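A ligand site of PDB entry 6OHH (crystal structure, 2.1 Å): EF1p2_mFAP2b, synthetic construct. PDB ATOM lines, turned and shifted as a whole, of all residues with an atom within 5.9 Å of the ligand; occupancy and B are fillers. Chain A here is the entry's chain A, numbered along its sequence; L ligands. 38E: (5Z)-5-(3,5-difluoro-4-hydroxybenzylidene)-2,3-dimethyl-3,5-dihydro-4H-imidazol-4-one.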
ATOM      1  N   VAL A  17     -19.899   0.613  17.376  1.00  0.00           N
ATOM      2  CA  VAL A  17     -19.546   1.858  18.032  1.00  0.00           C
ATOM      3  C   VAL A  17     -19.727   3.014  17.042  1.00  0.00           C
ATOM      4  O   VAL A  17     -19.279   2.937  15.895  1.00  0.00           O
ATOM      5  CB  VAL A  17     -18.099   1.824  18.563  1.00  0.00           C
ATOM      6  CG1 VAL A  17     -17.740   3.147  19.223  1.00  0.00           C
ATOM      7  CG2 VAL A  17     -17.924   0.660  19.538  1.00  0.00           C
ATOM      8  N   THR A  18     -20.392   4.074  17.501  1.00  0.00           N
ATOM      9  CA  THR A  18     -20.490   5.325  16.774  1.00  0.00           C
ATOM     10  C   THR A  18     -20.082   6.442  17.718  1.00  0.00           C
ATOM     11  O   THR A  18     -20.413   6.407  18.904  1.00  0.00           O
ATOM     12  CB  THR A  18     -21.906   5.594  16.245  1.00  0.00           C
ATOM     13  OG1 THR A  18     -22.829   5.534  17.335  1.00  0.00           O
ATOM     14  CG2 THR A  18     -22.294   4.553  15.190  1.00  0.00           C
ATOM     15  N   MET A  19     -19.344   7.421  17.207  1.00  0.00           N
ATOM     16  CA  MET A  19     -18.863   8.502  18.042  1.00  0.00           C
ATOM     17  C   MET A  19     -19.055   9.845  17.354  1.00  0.00           C
ATOM     18  O   MET A  19     -19.359   9.924  16.158  1.00  0.00           O
ATOM     19  CB  MET A  19     -17.378   8.335  18.398  1.00  0.00           C
ATOM     20  CG  MET A  19     -17.018   7.081  19.198  1.00  0.00           C
ATOM     21  SD  MET A  19     -15.327   7.200  19.784  1.00  0.00           S
ATOM     22  CE  MET A  19     -15.023   5.515  20.349  1.00  0.00           C
ATOM     23  N   THR A  20     -18.854  10.894  18.135  1.00  0.00           N
ATOM     24  CA  THR A  20     -18.816  12.267  17.677  1.00  0.00           C
ATOM     25  C   THR A  20     -17.666  12.934  18.419  1.00  0.00           C
ATOM     26  O   THR A  20     -17.521  12.722  19.627  1.00  0.00           O
ATOM     27  CB  THR A  20     -20.121  13.026  17.962  1.00  0.00           C
ATOM     28  OG1 THR A  20     -21.228  12.357  17.349  1.00  0.00           O
ATOM     29  CG2 THR A  20     -20.025  14.439  17.404  1.00  0.00           C
ATOM     30  N   ASN A  21     -16.851  13.705  17.722  1.00  0.00           N
ATOM     31  CA  ASN A  21     -15.784  14.419  18.397  1.00  0.00           C
ATOM     32  C   ASN A  21     -16.125  15.903  18.483  1.00  0.00           C
ATOM     33  O   ASN A  21     -17.113  16.377  17.918  1.00  0.00           O
ATOM     34  CB  ASN A  21     -14.413  14.181  17.725  1.00  0.00           C
ATOM     35  CG  ASN A  21     -14.333  14.712  16.297  1.00  0.00           C
ATOM     36  OD1 ASN A  21     -14.943  15.720  15.939  1.00  0.00           O
ATOM     37  ND2 ASN A  21     -13.544  14.029  15.469  1.00  0.00           N
ATOM     38  N   GLN A  25     -16.945  15.989  13.739  1.00  0.00           N
ATOM     39  CA  GLN A  25     -16.873  14.801  12.926  1.00  0.00           C
ATOM     40  C   GLN A  25     -17.575  13.636  13.632  1.00  0.00           C
ATOM     41  O   GLN A  25     -17.791  13.661  14.844  1.00  0.00           O
ATOM     42  CB  GLN A  25     -15.418  14.423  12.634  1.00  0.00           C
ATOM     43  CG  GLN A  25     -14.719  15.293  11.619  1.00  0.00           C
ATOM     44  CD  GLN A  25     -13.206  15.253  11.764  1.00  0.00           C
ATOM     45  OE1 GLN A  25     -12.682  14.807  12.785  1.00  0.00           O
ATOM     46  NE2 GLN A  25     -12.496  15.691  10.730  1.00  0.00           N
ATOM     47  N   THR A  26     -17.912  12.615  12.852  1.00  0.00           N
ATOM     48  CA  THR A  26     -18.496  11.402  13.402  1.00  0.00           C
ATOM     49  C   THR A  26     -17.657  10.208  12.985  1.00  0.00           C
ATOM     50  O   THR A  26     -16.761  10.315  12.139  1.00  0.00           O
ATOM     51  CB  THR A  26     -19.946  11.200  12.943  1.00  0.00           C
ATOM     52  OG1 THR A  26     -20.010  11.316  11.516  1.00  0.00           O
ATOM     53  CG2 THR A  26     -20.844  12.267  13.564  1.00  0.00           C
ATOM     54  N   SER A  27     -17.960   9.052  13.569  1.00  0.00           N
ATOM     55  CA  SER A  27     -17.231   7.832  13.245  1.00  0.00           C
ATOM     56  C   SER A  27     -18.157   6.628  13.398  1.00  0.00           C
ATOM     57  O   SER A  27     -19.164   6.684  14.105  1.00  0.00           O
ATOM     58  CB  SER A  27     -15.996   7.676  14.131  1.00  0.00           C
ATOM     59  OG  SER A  27     -16.373   7.341  15.453  1.00  0.00           O
ATOM     60  N   GLN A  28     -17.784   5.549  12.722  1.00  0.00           N
ATOM     61  CA  GLN A  28     -18.488   4.272  12.792  1.00  0.00           C
ATOM     62  C   GLN A  28     -17.452   3.156  12.794  1.00  0.00           C
ATOM     63  O   GLN A  28     -16.395   3.277  12.159  1.00  0.00           O
ATOM     64  CB  GLN A  28     -19.464   4.097  11.620  1.00  0.00           C
ATOM     65  CG  GLN A  28     -18.750   3.975  10.275  1.00  0.00           C
ATOM     66  CD  GLN A  28     -19.675   3.619   9.128  1.00  0.00           C
ATOM     67  OE1 GLN A  28     -19.459   2.613   8.445  1.00  0.00           O
ATOM     68  NE2 GLN A  28     -20.697   4.433   8.913  1.00  0.00           N
ATOM     69  N   GLY A  29     -17.745   2.087  13.524  1.00  0.00           N
ATOM     70  CA  GLY A  29     -16.774   1.011  13.635  1.00  0.00           C
ATOM     71  C   GLY A  29     -17.176   0.021  14.716  1.00  0.00           C
ATOM     72  O   GLY A  29     -18.354  -0.089  15.069  1.00  0.00           O
ATOM     73  N   GLN A  30     -16.181  -0.707  15.218  1.00  0.00           N
ATOM     74  CA  GLN A  30     -16.412  -1.751  16.201  1.00  0.00           C
ATOM     75  C   GLN A  30     -15.386  -1.689  17.329  1.00  0.00           C
ATOM     76  O   GLN A  30     -14.252  -1.245  17.132  1.00  0.00           O
ATOM     77  CB  GLN A  30     -16.344  -3.154  15.573  1.00  0.00           C
ATOM     78  CG  GLN A  30     -17.479  -3.487  14.627  1.00  0.00           C
ATOM     79  CD  GLN A  30     -17.291  -2.825  13.273  1.00  0.00           C
ATOM     80  OE1 GLN A  30     -16.156  -2.565  12.845  1.00  0.00           O
ATOM     81  NE2 GLN A  30     -18.386  -2.541  12.581  1.00  0.00           N
ATOM     82  N   TRP A  31     -15.794  -2.181  18.497  1.00  0.00           N
ATOM     83  CA  TRP A  31     -14.908  -2.472  19.612  1.00  0.00           C
ATOM     84  C   TRP A  31     -15.034  -3.953  19.913  1.00  0.00           C
ATOM     85  O   TRP A  31     -16.144  -4.492  19.901  1.00  0.00           O
ATOM     86  CB  TRP A  31     -15.262  -1.649  20.868  1.00  0.00           C
ATOM     87  CG  TRP A  31     -14.659  -0.284  20.925  1.00  0.00           C
ATOM     88  CD1 TRP A  31     -13.974   0.355  19.940  1.00  0.00           C
ATOM     89  CD2 TRP A  31     -14.729   0.631  22.028  1.00  0.00           C
ATOM     90  NE1 TRP A  31     -13.588   1.606  20.356  1.00  0.00           N
ATOM     91  CE2 TRP A  31     -14.043   1.806  21.636  1.00  0.00           C
ATOM     92  CE3 TRP A  31     -15.295   0.578  23.307  1.00  0.00           C
ATOM     93  CZ2 TRP A  31     -13.919   2.911  22.467  1.00  0.00           C
ATOM     94  CZ3 TRP A  31     -15.157   1.674  24.144  1.00  0.00           C
ATOM     95  CH2 TRP A  31     -14.478   2.826  23.718  1.00  0.00           C
ATOM     96  N   ALA A  45      -9.865  -1.813  18.424  1.00  0.00           N
ATOM     97  CA  ALA A  45     -10.816  -0.916  17.787  1.00  0.00           C
ATOM     98  C   ALA A  45     -10.510  -0.747  16.311  1.00  0.00           C
ATOM     99  O   ALA A  45      -9.350  -0.635  15.916  1.00  0.00           O
ATOM    100  CB  ALA A  45     -10.800   0.463  18.469  1.00  0.00           C
ATOM    101  N   GLN A  46     -11.568  -0.716  15.494  1.00  0.00           N
ATOM    102  CA  GLN A  46     -11.481  -0.431  14.075  1.00  0.00           C
ATOM    103  C   GLN A  46     -12.660   0.429  13.657  1.00  0.00           C
ATOM    104  O   GLN A  46     -13.732   0.366  14.267  1.00  0.00           O
ATOM    105  CB  GLN A  46     -11.459  -1.713  13.222  1.00  0.00           C
ATOM    106  CG  GLN A  46     -10.200  -2.544  13.383  1.00  0.00           C
ATOM    107  CD  GLN A  46     -10.130  -3.660  12.359  1.00  0.00           C
ATOM    108  OE1 GLN A  46     -11.114  -4.361  12.108  1.00  0.00           O
ATOM    109  NE2 GLN A  46      -8.955  -3.835  11.769  1.00  0.00           N
ATOM    110  N   GLY A  47     -12.466   1.237  12.626  1.00  0.00           N
ATOM    111  CA  GLY A  47     -13.529   2.081  12.126  1.00  0.00           C
ATOM    112  C   GLY A  47     -12.985   3.157  11.205  1.00  0.00           C
ATOM    113  O   GLY A  47     -11.842   3.108  10.764  1.00  0.00           O
ATOM    114  N   THR A  48     -13.849   4.139  10.939  1.00  0.00           N
ATOM    115  CA  THR A  48     -13.527   5.250  10.057  1.00  0.00           C
ATOM    116  C   THR A  48     -14.142   6.532  10.600  1.00  0.00           C
ATOM    117  O   THR A  48     -15.295   6.532  11.051  1.00  0.00           O
ATOM    118  CB  THR A  48     -14.040   5.003   8.633  1.00  0.00           C
ATOM    119  OG1 THR A  48     -13.805   3.636   8.272  1.00  0.00           O
ATOM    120  CG2 THR A  48     -13.345   5.920   7.643  1.00  0.00           C
ATOM    121  N   ILE A  49     -13.373   7.622  10.559  1.00  0.00           N
ATOM    122  CA  ILE A  49     -13.876   8.952  10.885  1.00  0.00           C
ATOM    123  C   ILE A  49     -14.567   9.555   9.662  1.00  0.00           C
ATOM    124  O   ILE A  49     -14.265   9.202   8.520  1.00  0.00           O
ATOM    125  CB  ILE A  49     -12.742   9.861  11.401  1.00  0.00           C
ATOM    126  CG1 ILE A  49     -11.920   9.136  12.474  1.00  0.00           C
ATOM    127  CG2 ILE A  49     -13.281  11.164  11.978  1.00  0.00           C
ATOM    128  CD1 ILE A  49     -10.874  10.014  13.134  1.00  0.00           C
ATOM    129  N   ILE A  55      -9.586   4.173  11.470  1.00  0.00           N
ATOM    130  CA  ILE A  55      -9.385   4.049  12.907  1.00  0.00           C
ATOM    131  C   ILE A  55      -8.829   2.662  13.202  1.00  0.00           C
ATOM    132  O   ILE A  55      -9.441   1.658  12.833  1.00  0.00           O
ATOM    133  CB  ILE A  55     -10.699   4.287  13.673  1.00  0.00           C
ATOM    134  CG1 ILE A  55     -11.320   5.625  13.271  1.00  0.00           C
ATOM    135  CG2 ILE A  55     -10.467   4.177  15.181  1.00  0.00           C
ATOM    136  CD1 ILE A  55     -12.582   5.948  14.006  1.00  0.00           C
ATOM    137  N   ILE A  73      -7.445   3.909  25.460  1.00  0.00           N
ATOM    138  CA  ILE A  73      -7.190   3.373  24.128  1.00  0.00           C
ATOM    139  C   ILE A  73      -6.162   4.239  23.403  1.00  0.00           C
ATOM    140  O   ILE A  73      -6.219   5.464  23.473  1.00  0.00           O
ATOM    141  CB  ILE A  73      -8.493   3.269  23.290  1.00  0.00           C
ATOM    142  CG1 ILE A  73      -9.522   2.408  24.007  1.00  0.00           C
ATOM    143  CG2 ILE A  73      -8.213   2.697  21.891  1.00  0.00           C
ATOM    144  CD1 ILE A  73     -10.731   2.087  23.168  1.00  0.00           C
ATOM    145  N   TYR A  75      -4.384   4.881  19.542  1.00  0.00           N
ATOM    146  CA  TYR A  75      -4.711   4.734  18.120  1.00  0.00           C
ATOM    147  C   TYR A  75      -3.478   4.912  17.250  1.00  0.00           C
ATOM    148  O   TYR A  75      -3.141   6.046  16.864  1.00  0.00           O
ATOM    149  CB  TYR A  75      -5.808   5.719  17.720  1.00  0.00           C
ATOM    150  CG  TYR A  75      -7.127   5.478  18.422  1.00  0.00           C
ATOM    151  CD1 TYR A  75      -7.445   6.126  19.617  1.00  0.00           C
ATOM    152  CD2 TYR A  75      -8.058   4.590  17.887  1.00  0.00           C
ATOM    153  CE1 TYR A  75      -8.652   5.901  20.244  1.00  0.00           C
ATOM    154  CE2 TYR A  75      -9.265   4.365  18.514  1.00  0.00           C
ATOM    155  CZ  TYR A  75      -9.563   5.023  19.688  1.00  0.00           C
ATOM    156  OH  TYR A  75     -10.775   4.786  20.309  1.00  0.00           O
ATOM    157  N   LEU A  78      -3.885   6.979  14.188  1.00  0.00           N
ATOM    158  CA  LEU A  78      -4.070   8.408  14.426  1.00  0.00           C
ATOM    159  C   LEU A  78      -2.901   8.979  15.218  1.00  0.00           C
ATOM    160  O   LEU A  78      -3.101   9.709  16.188  1.00  0.00           O
ATOM    161  CB  LEU A  78      -5.392   8.648  15.161  1.00  0.00           C
ATOM    162  CG  LEU A  78      -6.641   8.211  14.393  1.00  0.00           C
ATOM    163  CD1 LEU A  78      -7.898   8.386  15.232  1.00  0.00           C
ATOM    164  CD2 LEU A  78      -6.753   8.993  13.100  1.00  0.00           C
ATOM    165  N   ILE A  81      -2.577   8.838  19.292  1.00  0.00           N
ATOM    166  CA  ILE A  81      -3.367   9.613  20.246  1.00  0.00           C
ATOM    167  C   ILE A  81      -3.894   8.677  21.315  1.00  0.00           C
ATOM    168  O   ILE A  81      -4.103   7.484  21.074  1.00  0.00           O
ATOM    169  CB  ILE A  81      -4.523  10.365  19.576  1.00  0.00           C
ATOM    170  CG1 ILE A  81      -5.352   9.409  18.707  1.00  0.00           C
ATOM    171  CG2 ILE A  81      -4.026  11.575  18.798  1.00  0.00           C
ATOM    172  CD1 ILE A  81      -6.790   9.829  18.531  1.00  0.00           C
ATOM    173  N   TYR A 101      -9.323  13.051  24.326  1.00  0.00           N
ATOM    174  CA  TYR A 101      -8.083  12.554  23.755  1.00  0.00           C
ATOM    175  C   TYR A 101      -7.182  13.733  23.424  1.00  0.00           C
ATOM    176  O   TYR A 101      -7.627  14.863  23.275  1.00  0.00           O
ATOM    177  CB  TYR A 101      -8.330  11.726  22.493  1.00  0.00           C
ATOM    178  CG  TYR A 101      -8.819  12.565  21.340  1.00  0.00           C
ATOM    179  CD1 TYR A 101      -7.934  13.082  20.400  1.00  0.00           C
ATOM    180  CD2 TYR A 101     -10.170  12.868  21.205  1.00  0.00           C
ATOM    181  CE1 TYR A 101      -8.381  13.860  19.345  1.00  0.00           C
ATOM    182  CE2 TYR A 101     -10.622  13.653  20.155  1.00  0.00           C
ATOM    183  CZ  TYR A 101      -9.728  14.149  19.236  1.00  0.00           C
ATOM    184  OH  TYR A 101     -10.179  14.930  18.195  1.00  0.00           O
ATOM    185  N   LYS A 105      -2.477  13.680  16.400  1.00  0.00           N
ATOM    186  CA  LYS A 105      -3.535  13.069  15.583  1.00  0.00           C
ATOM    187  C   LYS A 105      -3.185  13.035  14.099  1.00  0.00           C
ATOM    188  O   LYS A 105      -3.484  12.051  13.422  1.00  0.00           O
ATOM    189  CB  LYS A 105      -4.863  13.794  15.820  1.00  0.00           C
ATOM    190  CG  LYS A 105      -6.054  12.955  15.415  1.00  0.00           C
ATOM    191  CD  LYS A 105      -7.377  13.662  15.687  1.00  0.00           C
ATOM    192  CE  LYS A 105      -8.542  12.686  15.560  1.00  0.00           C
ATOM    193  NZ  LYS A 105      -9.840  13.292  15.958  1.00  0.00           N
ATOM    194  N   LEU A 121     -14.887  13.507  23.261  1.00  0.00           N
ATOM    195  CA  LEU A 121     -15.323  12.342  22.500  1.00  0.00           C
ATOM    196  C   LEU A 121     -16.536  11.744  23.209  1.00  0.00           C
ATOM    197  O   LEU A 121     -16.463  11.453  24.397  1.00  0.00           O
ATOM    198  CB  LEU A 121     -14.219  11.285  22.421  1.00  0.00           C
ATOM    199  CG  LEU A 121     -13.418  11.015  21.146  1.00  0.00           C
ATOM    200  CD1 LEU A 121     -12.544   9.771  21.366  1.00  0.00           C
ATOM    201  CD2 LEU A 121     -14.306  10.854  19.923  1.00  0.00           C
HETATM  202  F1  38E L   1     -14.204  10.489  15.732  1.00  0.00           F
HETATM  203  C2  38E L   1     -13.216   9.834  16.386  1.00  0.00           C
HETATM  204  C1  38E L   1     -12.059  10.528  16.721  1.00  0.00           C
HETATM  205  O1  38E L   1     -11.930  11.828  16.383  1.00  0.00           O
HETATM  206  C3  38E L   1     -13.370   8.497  16.720  1.00  0.00           C
HETATM  207  C4  38E L   1     -12.332   7.846  17.413  1.00  0.00           C
HETATM  208  C5  38E L   1     -11.157   8.555  17.719  1.00  0.00           C
HETATM  209  C   38E L   1     -11.029   9.879  17.383  1.00  0.00           C
HETATM  210  F   38E L   1      -9.906  10.557  17.692  1.00  0.00           F
HETATM  211  C6  38E L   1     -12.371   6.425  17.778  1.00  0.00           C
HETATM  212  C7  38E L   1     -13.301   5.485  17.375  1.00  0.00           C
HETATM  213  C9  38E L   1     -13.270   4.059  17.749  1.00  0.00           C
HETATM  214  O   38E L   1     -12.439   3.510  18.446  1.00  0.00           O
HETATM  215  N1  38E L   1     -14.347   3.503  17.167  1.00  0.00           N
HETATM  216  C10 38E L   1     -14.753   2.098  17.231  1.00  0.00           C
HETATM  217  C8  38E L   1     -15.005   4.475  16.481  1.00  0.00           C
HETATM  218  N   38E L   1     -14.417   5.626  16.601  1.00  0.00           N
HETATM  219  C11 38E L   1     -16.272   4.214  15.704  1.00  0.00           C
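The side-chain amino group of Lys 105 sits at hydrogen-bond distance from the side-chain hydroxyl of Tyr 101, at 2.8 Å. The backbone carbonyl oxygen (O) of Ile 81 lies within hydrogen-bond range of the backbone NH (N) of Tyr 75, at 3.0 Å. N of Ser 27 is in hydrogen-bond range of O of Met 19 (3.1 Å). The side-chain amide oxygen of Gln 25 is in hydrogen-bond range of the side-chain amide nitrogen of Asn 21, 2.9 Å away. The backbone carbonyl oxygen (O) of Gly 47 is in hydrogen-bond range of the backbone NH (N) of Ile 55, 2.6 Å away. The backbone carbonyl oxygen (O) of Gly 29 is in hydrogen-bond range of the backbone NH (N) of Val 17 (2.9 Å). O of Gln 28 lies within hydrogen-bond range of N of Thr 48, at 3.0 Å. The backbone NH (N) of Gln 30 sits at hydrogen-bond distance from the backbone carbonyl oxygen (O) of Gln 46, at 2.8 Å.
The side-chain sulfur (SD) of Met 19 sits close to a nitrogen (N) of the ligand. Residues that only touch the ligand: Ile 55, Val 17, Ile 81, Gln 28, Gln 30, Gly 29, Ala 45, Gln 46, Ile 49, Leu 121, Leu 78 and Tyr 101. Hydrophobic or aromatic side chains within 4 Å of the ligand: Val 17, Met 19, Trp 31, Ala 45, Ile 49, Ile 55, Tyr 75, Leu 78, Ile 81, Tyr 101 and Leu 121. The nearest printed residue that does not touch the ligand is Thr 26 (4.4 Å).
The side-chain amino group of Lys 105 sits at hydrogen-bond distance from an oxygen (O1) of the ligand (2.6 Å). The side-chain hydroxyl (OH) of Tyr 75 sits at hydrogen-bond distance from an oxygen (O) of the ligand. A nitrogen (N) of the ligand is in hydrogen-bond range of the side-chain hydroxyl (OG) of Ser 27 (2.8 Å). The side-chain amide nitrogen of Asn 21 is in hydrogen-bond range of an oxygen (O1) of the ligand, 2.9 Å away. The indole nitrogen (NE1) of Trp 31 lies within hydrogen-bond range of an oxygen (O) of the ligand, 2.9 Å away.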
